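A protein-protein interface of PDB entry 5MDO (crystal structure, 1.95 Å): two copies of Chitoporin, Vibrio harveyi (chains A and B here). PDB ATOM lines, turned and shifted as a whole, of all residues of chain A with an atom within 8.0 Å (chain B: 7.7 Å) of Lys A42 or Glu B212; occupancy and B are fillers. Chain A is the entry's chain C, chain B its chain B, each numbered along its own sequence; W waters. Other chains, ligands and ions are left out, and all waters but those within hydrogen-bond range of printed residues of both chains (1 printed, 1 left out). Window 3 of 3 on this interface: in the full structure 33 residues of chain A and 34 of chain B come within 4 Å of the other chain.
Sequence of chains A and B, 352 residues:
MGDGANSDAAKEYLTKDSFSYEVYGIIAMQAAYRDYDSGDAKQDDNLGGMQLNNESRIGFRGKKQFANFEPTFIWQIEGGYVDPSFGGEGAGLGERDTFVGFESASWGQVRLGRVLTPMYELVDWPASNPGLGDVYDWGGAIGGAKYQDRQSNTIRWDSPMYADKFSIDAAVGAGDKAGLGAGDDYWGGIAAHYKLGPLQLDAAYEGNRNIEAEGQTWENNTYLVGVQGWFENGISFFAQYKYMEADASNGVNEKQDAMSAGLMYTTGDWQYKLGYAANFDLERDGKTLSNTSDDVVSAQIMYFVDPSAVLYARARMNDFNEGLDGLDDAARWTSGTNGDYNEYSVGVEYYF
Of the printed residues of chain B, Leu A47 touches Gly B181 (3.5 Å). Printed residues of chain A within 4 Å of Gly B183: Asp A45 (3.6 Å) and Asn A46 (3.2 Å). Asp A40 touches none of the printed residues of chain B.
The side-chain amino group of Lys B177 lies within salt-bridge range of the side-chain carboxylate of Glu B212. The backbone NH (N) of Ala B182 sits at hydrogen-bond distance from the backbone carbonyl oxygen (O) of Lys B177, 2.9 Å away. The side-chain amino group (NZ) of Lys A42 sits at hydrogen-bond distance from the side-chain amide oxygen (OD1) of Asn A46 (2.9 Å). OD1 of Asp A40 lies within hydrogen-bond range of N of Lys A42, at 3.1 Å. The backbone carbonyl oxygen (O) of Asp B184 lies within hydrogen-bond range of the side-chain amide nitrogen (ND2) of Asn B210 (3.1 Å).
Of the 11 printed residues of chain A, 4 touch a printed residue of chain B. Among the printed residues, Asp or Glu carboxylates within 4 Å of a Lys or Arg side-chain nitrogen of the other chain: Lys A42 with Glu B212.
No position is printed for both chains.
Water W1 lies within hydrogen-bond range of the side-chain carboxylate (OD2) of Asp A45 (2.7 Å), the side-chain carboxylate (OD2) of Asp B184 (2.9 Å) and the side-chain amino group (NZ) of Lys A42 (3.4 Å).
Among the printed residues, merely in contact across the chains: Asn A46 with Ala B182 (3.6 Å), Asp A45 with Gly B183 (3.6 Å) and Asp A45 with Asp B184 (3.8 Å).
N of Leu A47 lies within hydrogen-bond range of O of Gly B181. O of Asn A46 lies close to O of Gly B183, 3.3 Å away. The backbone carbonyl oxygen (O) of Asn A46 lies close to the backbone carbonyl oxygen (O) of Gly B181 (3.2 Å). OE2 of Glu B212 lies within salt-bridge range of NZ of Lys A42 (2.8 Å).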
ATOM      1  N   SER A  38      -8.654 -33.454 -15.550  1.00  0.00           N
ATOM      2  CA  SER A  38      -7.525 -33.520 -14.642  1.00  0.00           C
ATOM      3  C   SER A  38      -7.924 -33.138 -13.228  1.00  0.00           C
ATOM      4  O   SER A  38      -7.141 -33.350 -12.345  1.00  0.00           O
ATOM      5  CB  SER A  38      -6.404 -32.566 -15.085  1.00  0.00           C
ATOM      6  OG  SER A  38      -6.898 -31.236 -15.021  1.00  0.00           O
ATOM      7  N   GLY A  39      -9.098 -32.610 -12.984  1.00  0.00           N
ATOM      8  CA  GLY A  39      -9.400 -31.975 -11.691  1.00  0.00           C
ATOM      9  C   GLY A  39      -9.182 -30.454 -11.668  1.00  0.00           C
ATOM     10  O   GLY A  39      -9.632 -29.781 -10.755  1.00  0.00           O
ATOM     11  N   ASP A  40      -8.516 -29.876 -12.665  1.00  0.00           N
ATOM     12  CA  ASP A  40      -8.263 -28.398 -12.735  1.00  0.00           C
ATOM     13  C   ASP A  40      -8.741 -27.933 -14.131  1.00  0.00           C
ATOM     14  O   ASP A  40      -8.168 -28.377 -15.160  1.00  0.00           O
ATOM     15  CB  ASP A  40      -6.755 -28.254 -12.519  1.00  0.00           C
ATOM     16  CG  ASP A  40      -6.204 -26.837 -12.780  1.00  0.00           C
ATOM     17  OD1 ASP A  40      -6.777 -26.002 -13.474  1.00  0.00           O
ATOM     18  OD2 ASP A  40      -5.073 -26.634 -12.356  1.00  0.00           O
ATOM     19  N   ALA A  41      -9.782 -27.127 -14.158  1.00  0.00           N
ATOM     20  CA  ALA A  41     -10.497 -26.703 -15.384  1.00  0.00           C
ATOM     21  C   ALA A  41      -9.560 -25.889 -16.360  1.00  0.00           C
ATOM     22  O   ALA A  41      -9.585 -26.112 -17.568  1.00  0.00           O
ATOM     23  CB  ALA A  41     -11.685 -25.888 -15.037  1.00  0.00           C
ATOM     24  N   LYS A  42      -8.642 -25.112 -15.804  1.00  0.00           N
ATOM     25  CA  LYS A  42      -7.650 -24.372 -16.606  1.00  0.00           C
ATOM     26  C   LYS A  42      -6.653 -25.336 -17.278  1.00  0.00           C
ATOM     27  O   LYS A  42      -6.377 -25.227 -18.499  1.00  0.00           O
ATOM     28  CB  LYS A  42      -6.963 -23.288 -15.755  1.00  0.00           C
ATOM     29  CG  LYS A  42      -5.898 -22.461 -16.502  1.00  0.00           C
ATOM     30  CD  LYS A  42      -6.507 -21.737 -17.698  1.00  0.00           C
ATOM     31  CE  LYS A  42      -5.559 -20.644 -18.284  1.00  0.00           C
ATOM     32  NZ  LYS A  42      -5.513 -20.798 -19.777  1.00  0.00           N
ATOM     33  N   GLN A  43      -6.137 -26.313 -16.516  1.00  0.00           N
ATOM     34  CA  GLN A  43      -5.252 -27.260 -17.069  1.00  0.00           C
ATOM     35  C   GLN A  43      -5.961 -28.063 -18.182  1.00  0.00           C
ATOM     36  O   GLN A  43      -5.352 -28.347 -19.175  1.00  0.00           O
ATOM     37  CB  GLN A  43      -4.644 -28.178 -15.960  1.00  0.00           C
ATOM     38  CG  GLN A  43      -3.726 -29.288 -16.423  1.00  0.00           C
ATOM     39  CD  GLN A  43      -3.415 -30.305 -15.269  1.00  0.00           C
ATOM     40  OE1 GLN A  43      -3.427 -29.924 -14.107  1.00  0.00           O
ATOM     41  NE2 GLN A  43      -3.146 -31.564 -15.596  1.00  0.00           N
ATOM     42  N   ASP A  44      -7.217 -28.427 -17.976  1.00  0.00           N
ATOM     43  CA  ASP A  44      -8.006 -29.117 -18.991  1.00  0.00           C
ATOM     44  C   ASP A  44      -8.129 -28.307 -20.309  1.00  0.00           C
ATOM     45  O   ASP A  44      -7.969 -28.850 -21.411  1.00  0.00           O
ATOM     46  CB  ASP A  44      -9.421 -29.407 -18.493  1.00  0.00           C
ATOM     47  CG  ASP A  44      -9.461 -30.402 -17.325  1.00  0.00           C
ATOM     48  OD1 ASP A  44      -8.484 -31.133 -17.092  1.00  0.00           O
ATOM     49  OD2 ASP A  44     -10.538 -30.513 -16.718  1.00  0.00           O
ATOM     50  N   ASP A  45      -8.383 -27.018 -20.165  1.00  0.00           N
ATOM     51  CA  ASP A  45      -8.448 -26.095 -21.303  1.00  0.00           C
ATOM     52  C   ASP A  45      -7.099 -26.003 -22.002  1.00  0.00           C
ATOM     53  O   ASP A  45      -7.051 -26.028 -23.245  1.00  0.00           O
ATOM     54  CB  ASP A  45      -8.797 -24.654 -20.864  1.00  0.00           C
ATOM     55  CG  ASP A  45     -10.184 -24.524 -20.359  1.00  0.00           C
ATOM     56  OD1 ASP A  45     -11.032 -25.418 -20.609  1.00  0.00           O
ATOM     57  OD2 ASP A  45     -10.438 -23.474 -19.721  1.00  0.00           O
ATOM     58  N   ASN A  46      -6.020 -25.958 -21.221  1.00  0.00           N
ATOM     59  CA  ASN A  46      -4.699 -25.883 -21.789  1.00  0.00           C
ATOM     60  C   ASN A  46      -4.276 -27.153 -22.559  1.00  0.00           C
ATOM     61  O   ASN A  46      -3.880 -27.072 -23.738  1.00  0.00           O
ATOM     62  CB  ASN A  46      -3.665 -25.545 -20.751  1.00  0.00           C
ATOM     63  CG  ASN A  46      -3.798 -24.159 -20.217  1.00  0.00           C
ATOM     64  OD1 ASN A  46      -4.523 -23.332 -20.698  1.00  0.00           O
ATOM     65  ND2 ASN A  46      -3.013 -23.896 -19.194  1.00  0.00           N
ATOM     66  N   LEU A  47      -4.353 -28.314 -21.900  1.00  0.00           N
ATOM     67  CA  LEU A  47      -3.891 -29.557 -22.509  1.00  0.00           C
ATOM     68  C   LEU A  47      -4.830 -30.104 -23.587  1.00  0.00           C
ATOM     69  O   LEU A  47      -4.388 -30.758 -24.517  1.00  0.00           O
ATOM     70  CB  LEU A  47      -3.776 -30.654 -21.434  1.00  0.00           C
ATOM     71  CG  LEU A  47      -2.665 -30.398 -20.397  1.00  0.00           C
ATOM     72  CD1 LEU A  47      -2.798 -31.432 -19.286  1.00  0.00           C
ATOM     73  CD2 LEU A  47      -1.314 -30.556 -21.032  1.00  0.00           C
ATOM     74  N   GLY A  48      -6.111 -29.833 -23.454  1.00  0.00           N
ATOM     75  CA  GLY A  48      -7.117 -30.311 -24.375  1.00  0.00           C
ATOM     76  C   GLY A  48      -7.358 -29.389 -25.583  1.00  0.00           C
ATOM     77  O   GLY A  48      -6.706 -28.339 -25.703  1.00  0.00           O
ATOM     78  N   GLY B 144      -1.880  -8.038 -27.469  1.00  0.00           N
ATOM     79  CA  GLY B 144      -2.484  -9.285 -27.903  1.00  0.00           C
ATOM     80  C   GLY B 144      -1.729  -9.873 -29.060  1.00  0.00           C
ATOM     81  O   GLY B 144      -0.528  -9.811 -29.096  1.00  0.00           O
ATOM     82  N   ALA B 145      -2.427 -10.344 -30.075  1.00  0.00           N
ATOM     83  CA  ALA B 145      -1.770 -10.857 -31.274  1.00  0.00           C
ATOM     84  C   ALA B 145      -2.454 -10.304 -32.500  1.00  0.00           C
ATOM     85  O   ALA B 145      -3.534 -10.777 -32.882  1.00  0.00           O
ATOM     86  CB  ALA B 145      -1.795 -12.384 -31.316  1.00  0.00           C
ATOM     87  N   LYS B 177       0.232 -20.957 -27.796  1.00  0.00           N
ATOM     88  CA  LYS B 177       0.222 -21.715 -26.547  1.00  0.00           C
ATOM     89  C   LYS B 177      -0.526 -23.061 -26.690  1.00  0.00           C
ATOM     90  O   LYS B 177      -0.028 -24.069 -26.152  1.00  0.00           O
ATOM     91  CB  LYS B 177      -0.394 -20.917 -25.425  1.00  0.00           C
ATOM     92  CG  LYS B 177       0.448 -19.636 -25.163  1.00  0.00           C
ATOM     93  CD  LYS B 177      -0.028 -19.103 -23.838  1.00  0.00           C
ATOM     94  CE  LYS B 177       0.810 -17.963 -23.292  1.00  0.00           C
ATOM     95  NZ  LYS B 177       0.373 -17.973 -21.844  1.00  0.00           N
ATOM     96  N   GLY B 181       0.027 -27.341 -25.793  1.00  0.00           N
ATOM     97  CA  GLY B 181      -0.811 -27.824 -24.699  1.00  0.00           C
ATOM     98  C   GLY B 181      -0.794 -26.882 -23.507  1.00  0.00           C
ATOM     99  O   GLY B 181      -1.035 -27.326 -22.368  1.00  0.00           O
ATOM    100  N   ALA B 182      -0.547 -25.580 -23.750  1.00  0.00           N
ATOM    101  CA  ALA B 182      -0.329 -24.596 -22.648  1.00  0.00           C
ATOM    102  C   ALA B 182      -1.353 -23.453 -22.708  1.00  0.00           C
ATOM    103  O   ALA B 182      -1.174 -22.448 -22.058  1.00  0.00           O
ATOM    104  CB  ALA B 182       1.164 -24.043 -22.731  1.00  0.00           C
ATOM    105  N   GLY B 183      -2.399 -23.581 -23.499  1.00  0.00           N
ATOM    106  CA  GLY B 183      -3.404 -22.495 -23.622  1.00  0.00           C
ATOM    107  C   GLY B 183      -4.515 -22.947 -24.550  1.00  0.00           C
ATOM    108  O   GLY B 183      -4.506 -24.119 -24.998  1.00  0.00           O
ATOM    109  N   ASP B 184      -5.437 -22.052 -24.813  1.00  0.00           N
ATOM    110  CA  ASP B 184      -6.617 -22.314 -25.620  1.00  0.00           C
ATOM    111  C   ASP B 184      -6.856 -21.238 -26.631  1.00  0.00           C
ATOM    112  O   ASP B 184      -7.967 -20.974 -27.080  1.00  0.00           O
ATOM    113  CB  ASP B 184      -7.829 -22.635 -24.737  1.00  0.00           C
ATOM    114  CG  ASP B 184      -8.237 -21.498 -23.855  1.00  0.00           C
ATOM    115  OD1 ASP B 184      -7.584 -20.442 -23.841  1.00  0.00           O
ATOM    116  OD2 ASP B 184      -9.257 -21.670 -23.169  1.00  0.00           O
ATOM    117  N   ASP B 185      -5.728 -20.599 -27.026  1.00  0.00           N
ATOM    118  CA  ASP B 185      -5.770 -19.583 -28.054  1.00  0.00           C
ATOM    119  C   ASP B 185      -6.088 -20.201 -29.390  1.00  0.00           C
ATOM    120  O   ASP B 185      -5.718 -21.376 -29.682  1.00  0.00           O
ATOM    121  CB  ASP B 185      -4.428 -18.706 -28.107  1.00  0.00           C
ATOM    122  CG  ASP B 185      -3.135 -19.498 -27.931  1.00  0.00           C
ATOM    123  OD1 ASP B 185      -3.146 -20.784 -27.831  1.00  0.00           O
ATOM    124  OD2 ASP B 185      -2.035 -18.853 -27.897  1.00  0.00           O
ATOM    125  N   ARG B 209      -8.162 -15.048 -30.740  1.00  0.00           N
ATOM    126  CA  ARG B 209      -8.983 -15.211 -29.530  1.00  0.00           C
ATOM    127  C   ARG B 209      -8.247 -15.956 -28.432  1.00  0.00           C
ATOM    128  O   ARG B 209      -7.321 -16.778 -28.724  1.00  0.00           O
ATOM    129  CB  ARG B 209     -10.274 -15.976 -29.868  1.00  0.00           C
ATOM    130  CG  ARG B 209     -11.117 -15.347 -30.977  1.00  0.00           C
ATOM    131  CD  ARG B 209     -11.819 -14.119 -30.488  1.00  0.00           C
ATOM    132  NE  ARG B 209     -12.697 -13.462 -31.481  1.00  0.00           N
ATOM    133  CZ  ARG B 209     -12.352 -12.505 -32.339  1.00  0.00           C
ATOM    134  NH1 ARG B 209     -11.096 -12.021 -32.414  1.00  0.00           N
ATOM    135  NH2 ARG B 209     -13.297 -11.981 -33.114  1.00  0.00           N
ATOM    136  N   ASN B 210      -8.587 -15.666 -27.175  1.00  0.00           N
ATOM    137  CA  ASN B 210      -8.005 -16.300 -26.004  1.00  0.00           C
ATOM    138  C   ASN B 210      -6.494 -16.103 -25.916  1.00  0.00           C
ATOM    139  O   ASN B 210      -5.738 -16.986 -25.458  1.00  0.00           O
ATOM    140  CB  ASN B 210      -8.339 -17.806 -25.978  1.00  0.00           C
ATOM    141  CG  ASN B 210      -9.810 -18.063 -25.709  1.00  0.00           C
ATOM    142  OD1 ASN B 210     -10.514 -17.192 -25.275  1.00  0.00           O
ATOM    143  ND2 ASN B 210     -10.252 -19.283 -25.920  1.00  0.00           N
ATOM    144  N   ILE B 211      -6.025 -14.936 -26.348  1.00  0.00           N
ATOM    145  CA  ILE B 211      -4.571 -14.656 -26.380  1.00  0.00           C
ATOM    146  C   ILE B 211      -4.162 -14.191 -24.954  1.00  0.00           C
ATOM    147  O   ILE B 211      -4.721 -13.226 -24.455  1.00  0.00           O
ATOM    148  CB  ILE B 211      -4.227 -13.523 -27.361  1.00  0.00           C
ATOM    149  CG1 ILE B 211      -4.632 -13.938 -28.782  1.00  0.00           C
ATOM    150  CG2 ILE B 211      -2.729 -13.123 -27.279  1.00  0.00           C
ATOM    151  CD1 ILE B 211      -3.815 -15.062 -29.356  1.00  0.00           C
ATOM    152  N   GLU B 212      -3.175 -14.824 -24.334  1.00  0.00           N
ATOM    153  CA  GLU B 212      -2.790 -14.476 -22.983  1.00  0.00           C
ATOM    154  C   GLU B 212      -1.509 -13.651 -22.997  1.00  0.00           C
ATOM    155  O   GLU B 212      -0.540 -14.051 -23.578  1.00  0.00           O
ATOM    156  CB  GLU B 212      -2.582 -15.744 -22.149  1.00  0.00           C
ATOM    157  CG  GLU B 212      -3.929 -16.406 -21.837  1.00  0.00           C
ATOM    158  CD  GLU B 212      -3.745 -17.774 -21.167  1.00  0.00           C
ATOM    159  OE1 GLU B 212      -2.657 -18.385 -21.237  1.00  0.00           O
ATOM    160  OE2 GLU B 212      -4.682 -18.243 -20.555  1.00  0.00           O
ATOM    161  N   ALA B 213      -1.551 -12.444 -22.470  1.00  0.00           N
ATOM    162  CA  ALA B 213      -0.384 -11.519 -22.516  1.00  0.00           C
ATOM    163  C   ALA B 213      -0.673 -10.392 -21.545  1.00  0.00           C
ATOM    164  O   ALA B 213      -1.833  -9.971 -21.352  1.00  0.00           O
ATOM    165  CB  ALA B 213      -0.133 -10.943 -23.944  1.00  0.00           C
ATOM    166  N   GLU B 214       0.384 -10.000 -20.838  1.00  0.00           N
ATOM    167  CA  GLU B 214       0.375  -8.843 -19.941  1.00  0.00           C
ATOM    168  C   GLU B 214      -0.632  -8.986 -18.821  1.00  0.00           C
ATOM    169  O   GLU B 214      -1.204  -8.003 -18.340  1.00  0.00           O
ATOM    170  CB  GLU B 214       0.099  -7.540 -20.771  1.00  0.00           C
ATOM    171  CG  GLU B 214       1.161  -7.311 -21.856  1.00  0.00           C
ATOM    172  CD  GLU B 214       0.827  -6.144 -22.818  1.00  0.00           C
ATOM    173  OE1 GLU B 214      -0.102  -5.334 -22.537  1.00  0.00           O
ATOM    174  OE2 GLU B 214       1.500  -6.053 -23.830  1.00  0.00           O
ATOM    175  N   GLY B 215      -0.876 -10.222 -18.421  1.00  0.00           N
ATOM    176  CA  GLY B 215      -1.820 -10.498 -17.297  1.00  0.00           C
ATOM    177  C   GLY B 215      -3.275 -10.495 -17.737  1.00  0.00           C
ATOM    178  O   GLY B 215      -4.155 -10.534 -16.905  1.00  0.00           O
ATOM    179  N   GLN B 216      -3.557 -10.406 -19.042  1.00  0.00           N
ATOM    180  CA  GLN B 216      -4.939 -10.335 -19.529  1.00  0.00           C
ATOM    181  C   GLN B 216      -5.146 -11.405 -20.588  1.00  0.00           C
ATOM    182  O   GLN B 216      -4.208 -12.018 -21.089  1.00  0.00           O
ATOM    183  CB  GLN B 216      -5.236  -9.023 -20.266  1.00  0.00           C
ATOM    184  CG  GLN B 216      -4.757  -7.754 -19.614  1.00  0.00           C
ATOM    185  CD  GLN B 216      -5.349  -7.571 -18.257  1.00  0.00           C
ATOM    186  OE1 GLN B 216      -6.494  -7.761 -18.026  1.00  0.00           O
ATOM    187  NE2 GLN B 216      -4.507  -7.180 -17.345  1.00  0.00           N
ATOM    188  N   THR B 217      -6.416 -11.586 -20.932  1.00  0.00           N
ATOM    189  CA  THR B 217      -6.798 -12.312 -22.114  1.00  0.00           C
ATOM    190  C   THR B 217      -7.262 -11.305 -23.178  1.00  0.00           C
ATOM    191  O   THR B 217      -8.040 -10.407 -22.878  1.00  0.00           O
ATOM    192  CB  THR B 217      -7.907 -13.337 -21.745  1.00  0.00           C
ATOM    193  OG1 THR B 217      -7.332 -14.242 -20.820  1.00  0.00           O
ATOM    194  CG2 THR B 217      -8.257 -14.162 -22.950  1.00  0.00           C
ATOM    195  N   TRP B 218      -6.820 -11.492 -24.403  1.00  0.00           N
ATOM    196  CA  TRP B 218      -7.137 -10.571 -25.470  1.00  0.00           C
ATOM    197  C   TRP B 218      -7.906 -11.204 -26.617  1.00  0.00           C
ATOM    198  O   TRP B 218      -7.701 -12.384 -26.954  1.00  0.00           O
ATOM    199  CB  TRP B 218      -5.810 -10.051 -26.070  1.00  0.00           C
ATOM    200  CG  TRP B 218      -4.920  -9.302 -25.157  1.00  0.00           C
ATOM    201  CD1 TRP B 218      -4.077  -9.820 -24.201  1.00  0.00           C
ATOM    202  CD2 TRP B 218      -4.699  -7.890 -25.150  1.00  0.00           C
ATOM    203  NE1 TRP B 218      -3.372  -8.817 -23.603  1.00  0.00           N
ATOM    204  CE2 TRP B 218      -3.721  -7.620 -24.162  1.00  0.00           C
ATOM    205  CE3 TRP B 218      -5.272  -6.822 -25.840  1.00  0.00           C
ATOM    206  CZ2 TRP B 218      -3.286  -6.323 -23.850  1.00  0.00           C
ATOM    207  CZ3 TRP B 218      -4.811  -5.507 -25.560  1.00  0.00           C
ATOM    208  CH2 TRP B 218      -3.828  -5.276 -24.549  1.00  0.00           C
ATOM    209  N   GLU B 219      -8.657 -10.363 -27.313  1.00  0.00           N
ATOM    210  CA  GLU B 219      -9.148 -10.642 -28.671  1.00  0.00           C
ATOM    211  C   GLU B 219      -8.629  -9.564 -29.597  1.00  0.00           C
ATOM    212  O   GLU B 219      -8.751  -8.360 -29.292  1.00  0.00           O
ATOM    213  CB  GLU B 219     -10.692 -10.627 -28.676  1.00  0.00           C
ATOM    214  CG  GLU B 219     -11.210 -11.644 -27.664  1.00  0.00           C
ATOM    215  CD  GLU B 219     -12.701 -11.950 -27.814  1.00  0.00           C
ATOM    216  OE1 GLU B 219     -13.429 -11.251 -28.590  1.00  0.00           O
ATOM    217  OE2 GLU B 219     -13.143 -12.896 -27.149  1.00  0.00           O
HETATM  218  O   HOH W   1      -8.837 -21.343 -20.279  1.00  0.00           O
